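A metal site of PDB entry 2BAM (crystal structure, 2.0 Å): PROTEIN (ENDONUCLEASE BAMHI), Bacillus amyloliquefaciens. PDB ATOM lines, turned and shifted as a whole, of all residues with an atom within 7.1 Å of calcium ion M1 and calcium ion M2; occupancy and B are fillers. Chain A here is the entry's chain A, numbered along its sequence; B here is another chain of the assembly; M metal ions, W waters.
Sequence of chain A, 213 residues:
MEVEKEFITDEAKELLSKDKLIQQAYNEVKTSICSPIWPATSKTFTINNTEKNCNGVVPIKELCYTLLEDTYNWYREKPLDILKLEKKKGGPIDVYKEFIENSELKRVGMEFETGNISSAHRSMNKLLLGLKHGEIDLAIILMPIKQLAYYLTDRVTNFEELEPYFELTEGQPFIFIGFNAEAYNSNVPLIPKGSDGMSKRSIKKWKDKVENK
Four residues have an atom within 4 Å of calcium ion M2: Glu 77, Asp 94, DG 4 of chain B and DG 5 of chain B. The nearest printed residue that does not touch calcium ion M2 is Glu 111 (4.3 Å).
Calcium ion M1 is bound by OP1 of DG 5 of chain B, at 2.3 Å. Calcium ion M1 is bound by O of Phe 112 (2.4 Å). Water W4 is bound to calcium ion M1, at 2.5 Å. Calcium ion M1 is bound by OD2 of Asp 94. Calcium ion M1 is bound by water W5 (2.7 Å). OE2 of Glu 111 is bound to calcium ion M1. Calcium ion M1 has six donor atoms within binding distance.
Four residues have an atom within 4 Å of calcium ion M1: Asp 94, Glu 111, Phe 112 and DG 5 of chain B. The nearest printed residue that does not touch calcium ion M1 is Tyr 65 (4.2 Å).
Calcium ion M2 is bound by the side-chain carboxylate (OD1) of Asp 94, OP1 of DG 5 of chain B, water W2, water W3 and the side-chain carboxylate (OE1) of Glu 77. Slightly farther from calcium ion M2 lies O3' of DG 4 of chain B (3.0 Å).
Water W4 bridges O5' of DG 5 of chain B (2.8 Å) and the side-chain carboxylate (OE2) of Glu 113 (2.9 Å). Water W2 bridges OE2 of Glu 77 and O of Pro 92.
OP2 of DG 5 of chain B lies within hydrogen-bond range of the side-chain hydroxyl (OG) of Ser 119 (3.4 Å). The side-chain hydroxyl (OH) of Tyr 65 sits close to the side-chain carboxylate (OD2) of Asp 94, at 3.0 Å. O of Asp 94 lies close to NE of Arg 76. NH2 of Arg 76 sits close to OE1 of Glu 77 (3.5 Å). OE2 of Glu 111 lies close to OG of Ser 123 (3.3 Å). The backbone NH of Leu 142 sits at hydrogen-bond distance from the backbone carbonyl oxygen of Glu 111 (2.9 Å). NZ of Lys 126 is in salt-bridge range of OP1 of DG 4 of chain B. OP1 of DG 4 of chain B sits at hydrogen-bond distance from the backbone NH of Gly 91 (2.7 Å).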
ATOM      1  N   LYS A  61     -17.521  23.775  20.624  1.00  0.00           N
ATOM      2  CA  LYS A  61     -18.689  24.270  21.336  1.00  0.00           C
ATOM      3  C   LYS A  61     -18.659  24.180  22.846  1.00  0.00           C
ATOM      4  O   LYS A  61     -19.403  24.886  23.521  1.00  0.00           O
ATOM      5  CB  LYS A  61     -19.948  23.544  20.859  1.00  0.00           C
ATOM      6  CG  LYS A  61     -19.963  22.079  21.224  1.00  0.00           C
ATOM      7  CD  LYS A  61     -21.146  21.343  20.647  1.00  0.00           C
ATOM      8  CE  LYS A  61     -20.701  20.306  19.611  1.00  0.00           C
ATOM      9  NZ  LYS A  61     -20.658  20.893  18.262  1.00  0.00           N
ATOM     10  N   TYR A  65     -20.859  26.624  25.611  1.00  0.00           N
ATOM     11  CA  TYR A  65     -22.009  26.060  26.309  1.00  0.00           C
ATOM     12  C   TYR A  65     -21.847  26.065  27.837  1.00  0.00           C
ATOM     13  O   TYR A  65     -22.823  26.199  28.575  1.00  0.00           O
ATOM     14  CB  TYR A  65     -22.295  24.653  25.814  1.00  0.00           C
ATOM     15  CG  TYR A  65     -23.010  24.600  24.488  1.00  0.00           C
ATOM     16  CD1 TYR A  65     -24.091  25.427  24.242  1.00  0.00           C
ATOM     17  CD2 TYR A  65     -22.626  23.691  23.505  1.00  0.00           C
ATOM     18  CE1 TYR A  65     -24.785  25.352  23.034  1.00  0.00           C
ATOM     19  CE2 TYR A  65     -23.326  23.611  22.304  1.00  0.00           C
ATOM     20  CZ  TYR A  65     -24.394  24.441  22.072  1.00  0.00           C
ATOM     21  OH  TYR A  65     -25.095  24.339  20.901  1.00  0.00           O
ATOM     22  N   ARG A  76     -30.134  24.647  27.750  1.00  0.00           N
ATOM     23  CA  ARG A  76     -29.710  23.881  26.563  1.00  0.00           C
ATOM     24  C   ARG A  76     -30.860  23.065  26.000  1.00  0.00           C
ATOM     25  O   ARG A  76     -31.790  22.716  26.726  1.00  0.00           O
ATOM     26  CB  ARG A  76     -28.561  22.896  26.874  1.00  0.00           C
ATOM     27  CG  ARG A  76     -27.147  23.343  26.491  1.00  0.00           C
ATOM     28  CD  ARG A  76     -26.963  23.759  25.033  1.00  0.00           C
ATOM     29  NE  ARG A  76     -26.972  22.679  24.051  1.00  0.00           N
ATOM     30  CZ  ARG A  76     -25.999  21.778  23.890  1.00  0.00           C
ATOM     31  NH1 ARG A  76     -24.917  21.798  24.671  1.00  0.00           N
ATOM     32  NH2 ARG A  76     -26.070  20.909  22.881  1.00  0.00           N
ATOM     33  N   GLU A  77     -30.775  22.737  24.722  1.00  0.00           N
ATOM     34  CA  GLU A  77     -31.771  21.936  24.043  1.00  0.00           C
ATOM     35  C   GLU A  77     -33.204  22.228  24.474  1.00  0.00           C
ATOM     36  O   GLU A  77     -33.896  21.369  25.008  1.00  0.00           O
ATOM     37  CB  GLU A  77     -31.453  20.455  24.229  1.00  0.00           C
ATOM     38  CG  GLU A  77     -30.128  20.058  23.579  1.00  0.00           C
ATOM     39  CD  GLU A  77     -30.104  20.385  22.098  1.00  0.00           C
ATOM     40  OE1 GLU A  77     -29.376  21.307  21.707  1.00  0.00           O
ATOM     41  OE2 GLU A  77     -30.825  19.713  21.325  1.00  0.00           O
ATOM     42  N   GLY A  91     -36.674  18.701  16.475  1.00  0.00           N
ATOM     43  CA  GLY A  91     -36.048  18.743  17.784  1.00  0.00           C
ATOM     44  C   GLY A  91     -35.973  20.163  18.346  1.00  0.00           C
ATOM     45  O   GLY A  91     -36.497  21.081  17.755  1.00  0.00           O
ATOM     46  N   PRO A  92     -35.288  20.347  19.488  1.00  0.00           N
ATOM     47  CA  PRO A  92     -35.134  21.619  20.183  1.00  0.00           C
ATOM     48  C   PRO A  92     -34.046  22.510  19.593  1.00  0.00           C
ATOM     49  O   PRO A  92     -33.275  22.083  18.672  1.00  0.00           O
ATOM     50  CB  PRO A  92     -34.729  21.203  21.550  1.00  0.00           C
ATOM     51  CG  PRO A  92     -33.881  20.022  21.282  1.00  0.00           C
ATOM     52  CD  PRO A  92     -34.672  19.276  20.255  1.00  0.00           C
ATOM     53  N   ILE A  93     -34.032  23.752  20.069  1.00  0.00           N
ATOM     54  CA  ILE A  93     -32.961  24.714  19.609  1.00  0.00           C
ATOM     55  C   ILE A  93     -31.857  24.593  20.673  1.00  0.00           C
ATOM     56  O   ILE A  93     -32.046  24.211  21.803  1.00  0.00           O
ATOM     57  CB  ILE A  93     -33.413  26.218  19.609  1.00  0.00           C
ATOM     58  CG1 ILE A  93     -33.993  26.676  20.968  1.00  0.00           C
ATOM     59  CG2 ILE A  93     -34.486  26.460  18.483  1.00  0.00           C
ATOM     60  CD1 ILE A  93     -34.402  28.146  20.965  1.00  0.00           C
ATOM     61  N   ASP A  94     -30.612  24.929  20.253  1.00  0.00           N
ATOM     62  CA  ASP A  94     -29.425  24.823  21.063  1.00  0.00           C
ATOM     63  C   ASP A  94     -29.551  25.454  22.448  1.00  0.00           C
ATOM     64  O   ASP A  94     -29.295  24.802  23.472  1.00  0.00           O
ATOM     65  CB  ASP A  94     -28.231  25.490  20.348  1.00  0.00           C
ATOM     66  CG  ASP A  94     -27.573  24.579  19.388  1.00  0.00           C
ATOM     67  OD1 ASP A  94     -27.762  23.349  19.500  1.00  0.00           O
ATOM     68  OD2 ASP A  94     -26.828  25.057  18.504  1.00  0.00           O
ATOM     69  N   VAL A  95     -29.889  26.730  22.514  1.00  0.00           N
ATOM     70  CA  VAL A  95     -30.013  27.425  23.808  1.00  0.00           C
ATOM     71  C   VAL A  95     -31.144  28.405  23.796  1.00  0.00           C
ATOM     72  O   VAL A  95     -31.557  28.935  22.755  1.00  0.00           O
ATOM     73  CB  VAL A  95     -28.706  28.167  24.164  1.00  0.00           C
ATOM     74  CG1 VAL A  95     -28.225  27.701  25.530  1.00  0.00           C
ATOM     75  CG2 VAL A  95     -27.610  27.976  23.127  1.00  0.00           C
ATOM     76  N   GLU A 111     -28.678  29.409  18.348  1.00  0.00           N
ATOM     77  CA  GLU A 111     -28.166  28.200  17.747  1.00  0.00           C
ATOM     78  C   GLU A 111     -26.697  28.444  17.475  1.00  0.00           C
ATOM     79  O   GLU A 111     -26.313  29.482  16.938  1.00  0.00           O
ATOM     80  CB  GLU A 111     -28.900  27.940  16.437  1.00  0.00           C
ATOM     81  CG  GLU A 111     -28.435  26.735  15.692  1.00  0.00           C
ATOM     82  CD  GLU A 111     -28.922  25.447  16.306  1.00  0.00           C
ATOM     83  OE1 GLU A 111     -29.943  25.477  17.023  1.00  0.00           O
ATOM     84  OE2 GLU A 111     -28.279  24.403  16.051  1.00  0.00           O
ATOM     85  N   PHE A 112     -25.871  27.487  17.903  1.00  0.00           N
ATOM     86  CA  PHE A 112     -24.418  27.540  17.679  1.00  0.00           C
ATOM     87  C   PHE A 112     -24.199  26.556  16.544  1.00  0.00           C
ATOM     88  O   PHE A 112     -24.545  25.386  16.668  1.00  0.00           O
ATOM     89  CB  PHE A 112     -23.670  27.073  18.930  1.00  0.00           C
ATOM     90  CG  PHE A 112     -22.212  26.776  18.689  1.00  0.00           C
ATOM     91  CD1 PHE A 112     -21.808  25.557  18.153  1.00  0.00           C
ATOM     92  CD2 PHE A 112     -21.242  27.718  18.997  1.00  0.00           C
ATOM     93  CE1 PHE A 112     -20.463  25.283  17.935  1.00  0.00           C
ATOM     94  CE2 PHE A 112     -19.885  27.437  18.783  1.00  0.00           C
ATOM     95  CZ  PHE A 112     -19.510  26.226  18.243  1.00  0.00           C
ATOM     96  N   GLU A 113     -23.560  26.993  15.466  1.00  0.00           N
ATOM     97  CA  GLU A 113     -23.362  26.088  14.347  1.00  0.00           C
ATOM     98  C   GLU A 113     -21.970  25.683  13.892  1.00  0.00           C
ATOM     99  O   GLU A 113     -21.180  26.486  13.459  1.00  0.00           O
ATOM    100  CB  GLU A 113     -24.134  26.593  13.122  1.00  0.00           C
ATOM    101  CG  GLU A 113     -25.608  26.163  13.041  1.00  0.00           C
ATOM    102  CD  GLU A 113     -25.807  24.707  12.640  1.00  0.00           C
ATOM    103  OE1 GLU A 113     -26.973  24.304  12.510  1.00  0.00           O
ATOM    104  OE2 GLU A 113     -24.833  23.942  12.465  1.00  0.00           O
ATOM    105  N   THR A 114     -21.694  24.401  14.010  1.00  0.00           N
ATOM    106  CA  THR A 114     -20.465  23.831  13.511  1.00  0.00           C
ATOM    107  C   THR A 114     -20.826  22.556  12.738  1.00  0.00           C
ATOM    108  O   THR A 114     -19.987  21.683  12.499  1.00  0.00           O
ATOM    109  CB  THR A 114     -19.410  23.535  14.622  1.00  0.00           C
ATOM    110  OG1 THR A 114     -20.032  22.945  15.767  1.00  0.00           O
ATOM    111  CG2 THR A 114     -18.637  24.810  14.991  1.00  0.00           C
ATOM    112  N   GLY A 115     -22.108  22.433  12.403  1.00  0.00           N
ATOM    113  CA  GLY A 115     -22.572  21.291  11.625  1.00  0.00           C
ATOM    114  C   GLY A 115     -22.460  21.744  10.178  1.00  0.00           C
ATOM    115  O   GLY A 115     -21.995  22.836   9.906  1.00  0.00           O
ATOM    116  N   SER A 119     -27.053  22.499   7.628  1.00  0.00           N
ATOM    117  CA  SER A 119     -27.644  22.390   8.945  1.00  0.00           C
ATOM    118  C   SER A 119     -27.978  23.780   9.483  1.00  0.00           C
ATOM    119  O   SER A 119     -28.939  23.940  10.244  1.00  0.00           O
ATOM    120  CB  SER A 119     -26.718  21.666   9.915  1.00  0.00           C
ATOM    121  OG  SER A 119     -27.212  21.709  11.229  1.00  0.00           O
ATOM    122  N   SER A 123     -31.385  25.547  11.262  1.00  0.00           N
ATOM    123  CA  SER A 123     -31.253  26.341  12.484  1.00  0.00           C
ATOM    124  C   SER A 123     -31.906  27.695  12.349  1.00  0.00           C
ATOM    125  O   SER A 123     -32.550  28.167  13.288  1.00  0.00           O
ATOM    126  CB  SER A 123     -29.793  26.526  12.805  1.00  0.00           C
ATOM    127  OG  SER A 123     -29.189  25.281  13.038  1.00  0.00           O
ATOM    128  N   LYS A 126     -35.735  27.182  12.102  1.00  0.00           N
ATOM    129  CA  LYS A 126     -36.335  26.815  13.383  1.00  0.00           C
ATOM    130  C   LYS A 126     -36.536  28.058  14.245  1.00  0.00           C
ATOM    131  O   LYS A 126     -37.577  28.238  14.858  1.00  0.00           O
ATOM    132  CB  LYS A 126     -35.466  25.794  14.115  1.00  0.00           C
ATOM    133  CG  LYS A 126     -36.034  25.320  15.417  1.00  0.00           C
ATOM    134  CD  LYS A 126     -35.208  24.213  16.030  1.00  0.00           C
ATOM    135  CE  LYS A 126     -35.241  22.946  15.195  1.00  0.00           C
ATOM    136  NZ  LYS A 126     -34.329  21.905  15.752  1.00  0.00           N
ATOM    137  N   LEU A 142     -24.524  31.430  15.848  1.00  0.00           N
ATOM    138  CA  LEU A 142     -23.078  31.546  16.010  1.00  0.00           C
ATOM    139  C   LEU A 142     -22.442  30.505  15.080  1.00  0.00           C
ATOM    140  O   LEU A 142     -22.884  29.375  15.040  1.00  0.00           O
ATOM    141  CB  LEU A 142     -22.687  31.259  17.443  1.00  0.00           C
ATOM    142  CG  LEU A 142     -23.467  31.991  18.524  1.00  0.00           C
ATOM    143  CD1 LEU A 142     -23.035  31.508  19.894  1.00  0.00           C
ATOM    144  CD2 LEU A 142     -23.283  33.478  18.382  1.00  0.00           C
ATOM    145  P    DG B   4     -33.785  18.314  14.419  1.00  0.00           P
ATOM    146  OP1  DG B   4     -34.854  19.296  14.605  1.00  0.00           O
ATOM    147  OP2  DG B   4     -33.515  17.768  13.069  1.00  0.00           O
ATOM    148  O5'  DG B   4     -32.444  18.940  14.991  1.00  0.00           O
ATOM    149  C5'  DG B   4     -32.205  18.852  16.381  1.00  0.00           C
ATOM    150  C4'  DG B   4     -30.730  18.606  16.653  1.00  0.00           C
ATOM    151  O4'  DG B   4     -30.349  17.254  16.278  1.00  0.00           O
ATOM    152  C3'  DG B   4     -29.885  19.524  15.773  1.00  0.00           C
ATOM    153  O3'  DG B   4     -28.651  19.749  16.403  1.00  0.00           O
ATOM    154  C2'  DG B   4     -29.644  18.688  14.540  1.00  0.00           C
ATOM    155  C1'  DG B   4     -29.445  17.327  15.181  1.00  0.00           C
ATOM    156  N9   DG B   4     -29.636  16.177  14.323  1.00  0.00           N
ATOM    157  C8   DG B   4     -30.658  15.988  13.420  1.00  0.00           C
ATOM    158  N7   DG B   4     -30.565  14.860  12.769  1.00  0.00           N
ATOM    159  C5   DG B   4     -29.409  14.280  13.261  1.00  0.00           C
ATOM    160  C6   DG B   4     -28.793  13.052  12.932  1.00  0.00           C
ATOM    161  O6   DG B   4     -29.148  12.226  12.109  1.00  0.00           O
ATOM    162  N1   DG B   4     -27.643  12.837  13.674  1.00  0.00           N
ATOM    163  C2   DG B   4     -27.134  13.694  14.613  1.00  0.00           C
ATOM    164  N2   DG B   4     -25.984  13.308  15.204  1.00  0.00           N
ATOM    165  N3   DG B   4     -27.698  14.858  14.938  1.00  0.00           N
ATOM    166  C4   DG B   4     -28.823  15.079  14.226  1.00  0.00           C
ATOM    167  P    DG B   5     -27.659  20.842  15.827  1.00  0.00           P
ATOM    168  OP1  DG B   5     -27.544  21.814  16.938  1.00  0.00           O
ATOM    169  OP2  DG B   5     -28.087  21.292  14.500  1.00  0.00           O
ATOM    170  O5'  DG B   5     -26.309  20.025  15.720  1.00  0.00           O
ATOM    171  C5'  DG B   5     -26.332  18.707  15.201  1.00  0.00           C
ATOM    172  C4'  DG B   5     -25.087  17.942  15.602  1.00  0.00           C
ATOM    173  O4'  DG B   5     -25.268  16.644  15.025  1.00  0.00           O
ATOM    174  C3'  DG B   5     -23.784  18.479  15.018  1.00  0.00           C
ATOM    175  O3'  DG B   5     -22.687  18.083  15.864  1.00  0.00           O
ATOM    176  C2'  DG B   5     -23.753  17.807  13.666  1.00  0.00           C
ATOM    177  C1'  DG B   5     -24.412  16.464  13.923  1.00  0.00           C
ATOM    178  N9   DG B   5     -25.237  16.008  12.816  1.00  0.00           N
ATOM    179  C8   DG B   5     -26.357  16.612  12.316  1.00  0.00           C
ATOM    180  N7   DG B   5     -26.871  15.963  11.304  1.00  0.00           N
ATOM    181  C5   DG B   5     -26.039  14.861  11.139  1.00  0.00           C
ATOM    182  C6   DG B   5     -26.086  13.799  10.186  1.00  0.00           C
ATOM    183  O6   DG B   5     -26.889  13.611   9.272  1.00  0.00           O
ATOM    184  N1   DG B   5     -25.037  12.909  10.379  1.00  0.00           N
ATOM    185  C2   DG B   5     -24.077  13.018  11.348  1.00  0.00           C
ATOM    186  N2   DG B   5     -23.160  12.057  11.362  1.00  0.00           N
ATOM    187  N3   DG B   5     -24.024  13.996  12.234  1.00  0.00           N
ATOM    188  C4   DG B   5     -25.026  14.881  12.068  1.00  0.00           C
ATOM    189  P    DA B   6     -21.222  18.734  15.663  1.00  0.00           P
ATOM    190  OP1  DA B   6     -20.509  18.604  16.958  1.00  0.00           O
ATOM    191  OP2  DA B   6     -21.331  20.061  15.033  1.00  0.00           O
ATOM    192  O5'  DA B   6     -20.475  17.745  14.657  1.00  0.00           O
ATOM    193  C5'  DA B   6     -20.990  16.422  14.439  1.00  0.00           C
ATOM    194  C4'  DA B   6     -19.980  15.542  13.746  1.00  0.00           C
ATOM    195  O4'  DA B   6     -20.658  14.941  12.611  1.00  0.00           O
ATOM    196  C3'  DA B   6     -18.740  16.209  13.164  1.00  0.00           C
ATOM    197  O3'  DA B   6     -17.670  15.251  13.183  1.00  0.00           O
ATOM    198  C2'  DA B   6     -19.206  16.599  11.761  1.00  0.00           C
ATOM    199  C1'  DA B   6     -20.146  15.451  11.401  1.00  0.00           C
ATOM    200  N9   DA B   6     -21.296  15.742  10.526  1.00  0.00           N
ATOM    201  C8   DA B   6     -22.094  16.855  10.517  1.00  0.00           C
ATOM    202  N7   DA B   6     -23.038  16.820   9.612  1.00  0.00           N
ATOM    203  C5   DA B   6     -22.848  15.600   8.977  1.00  0.00           C
ATOM    204  C6   DA B   6     -23.543  14.969   7.914  1.00  0.00           C
ATOM    205  N6   DA B   6     -24.595  15.496   7.281  1.00  0.00           N
ATOM    206  N1   DA B   6     -23.115  13.756   7.527  1.00  0.00           N
ATOM    207  C2   DA B   6     -22.058  13.220   8.158  1.00  0.00           C
ATOM    208  N3   DA B   6     -21.332  13.722   9.155  1.00  0.00           N
ATOM    209  C4   DA B   6     -21.779  14.927   9.532  1.00  0.00           C
HETATM  210 CA    CA M   1     -25.811  23.363  16.897  1.00  0.00          CA
HETATM  211 CA    CA M   2     -29.021  21.284  18.945  1.00  0.00          CA
HETATM  212  O   HOH W   1     -26.149  20.371  20.077  1.00  0.00           O
HETATM  213  O   HOH W   2     -31.373  20.293  18.868  1.00  0.00           O
HETATM  214  O   HOH W   3     -28.107  18.848  18.807  1.00  0.00           O
HETATM  215  O   HOH W   4     -25.028  22.282  14.807  1.00  0.00           O
HETATM  216  O   HOH W   5     -24.138  22.416  18.812  1.00  0.00           O
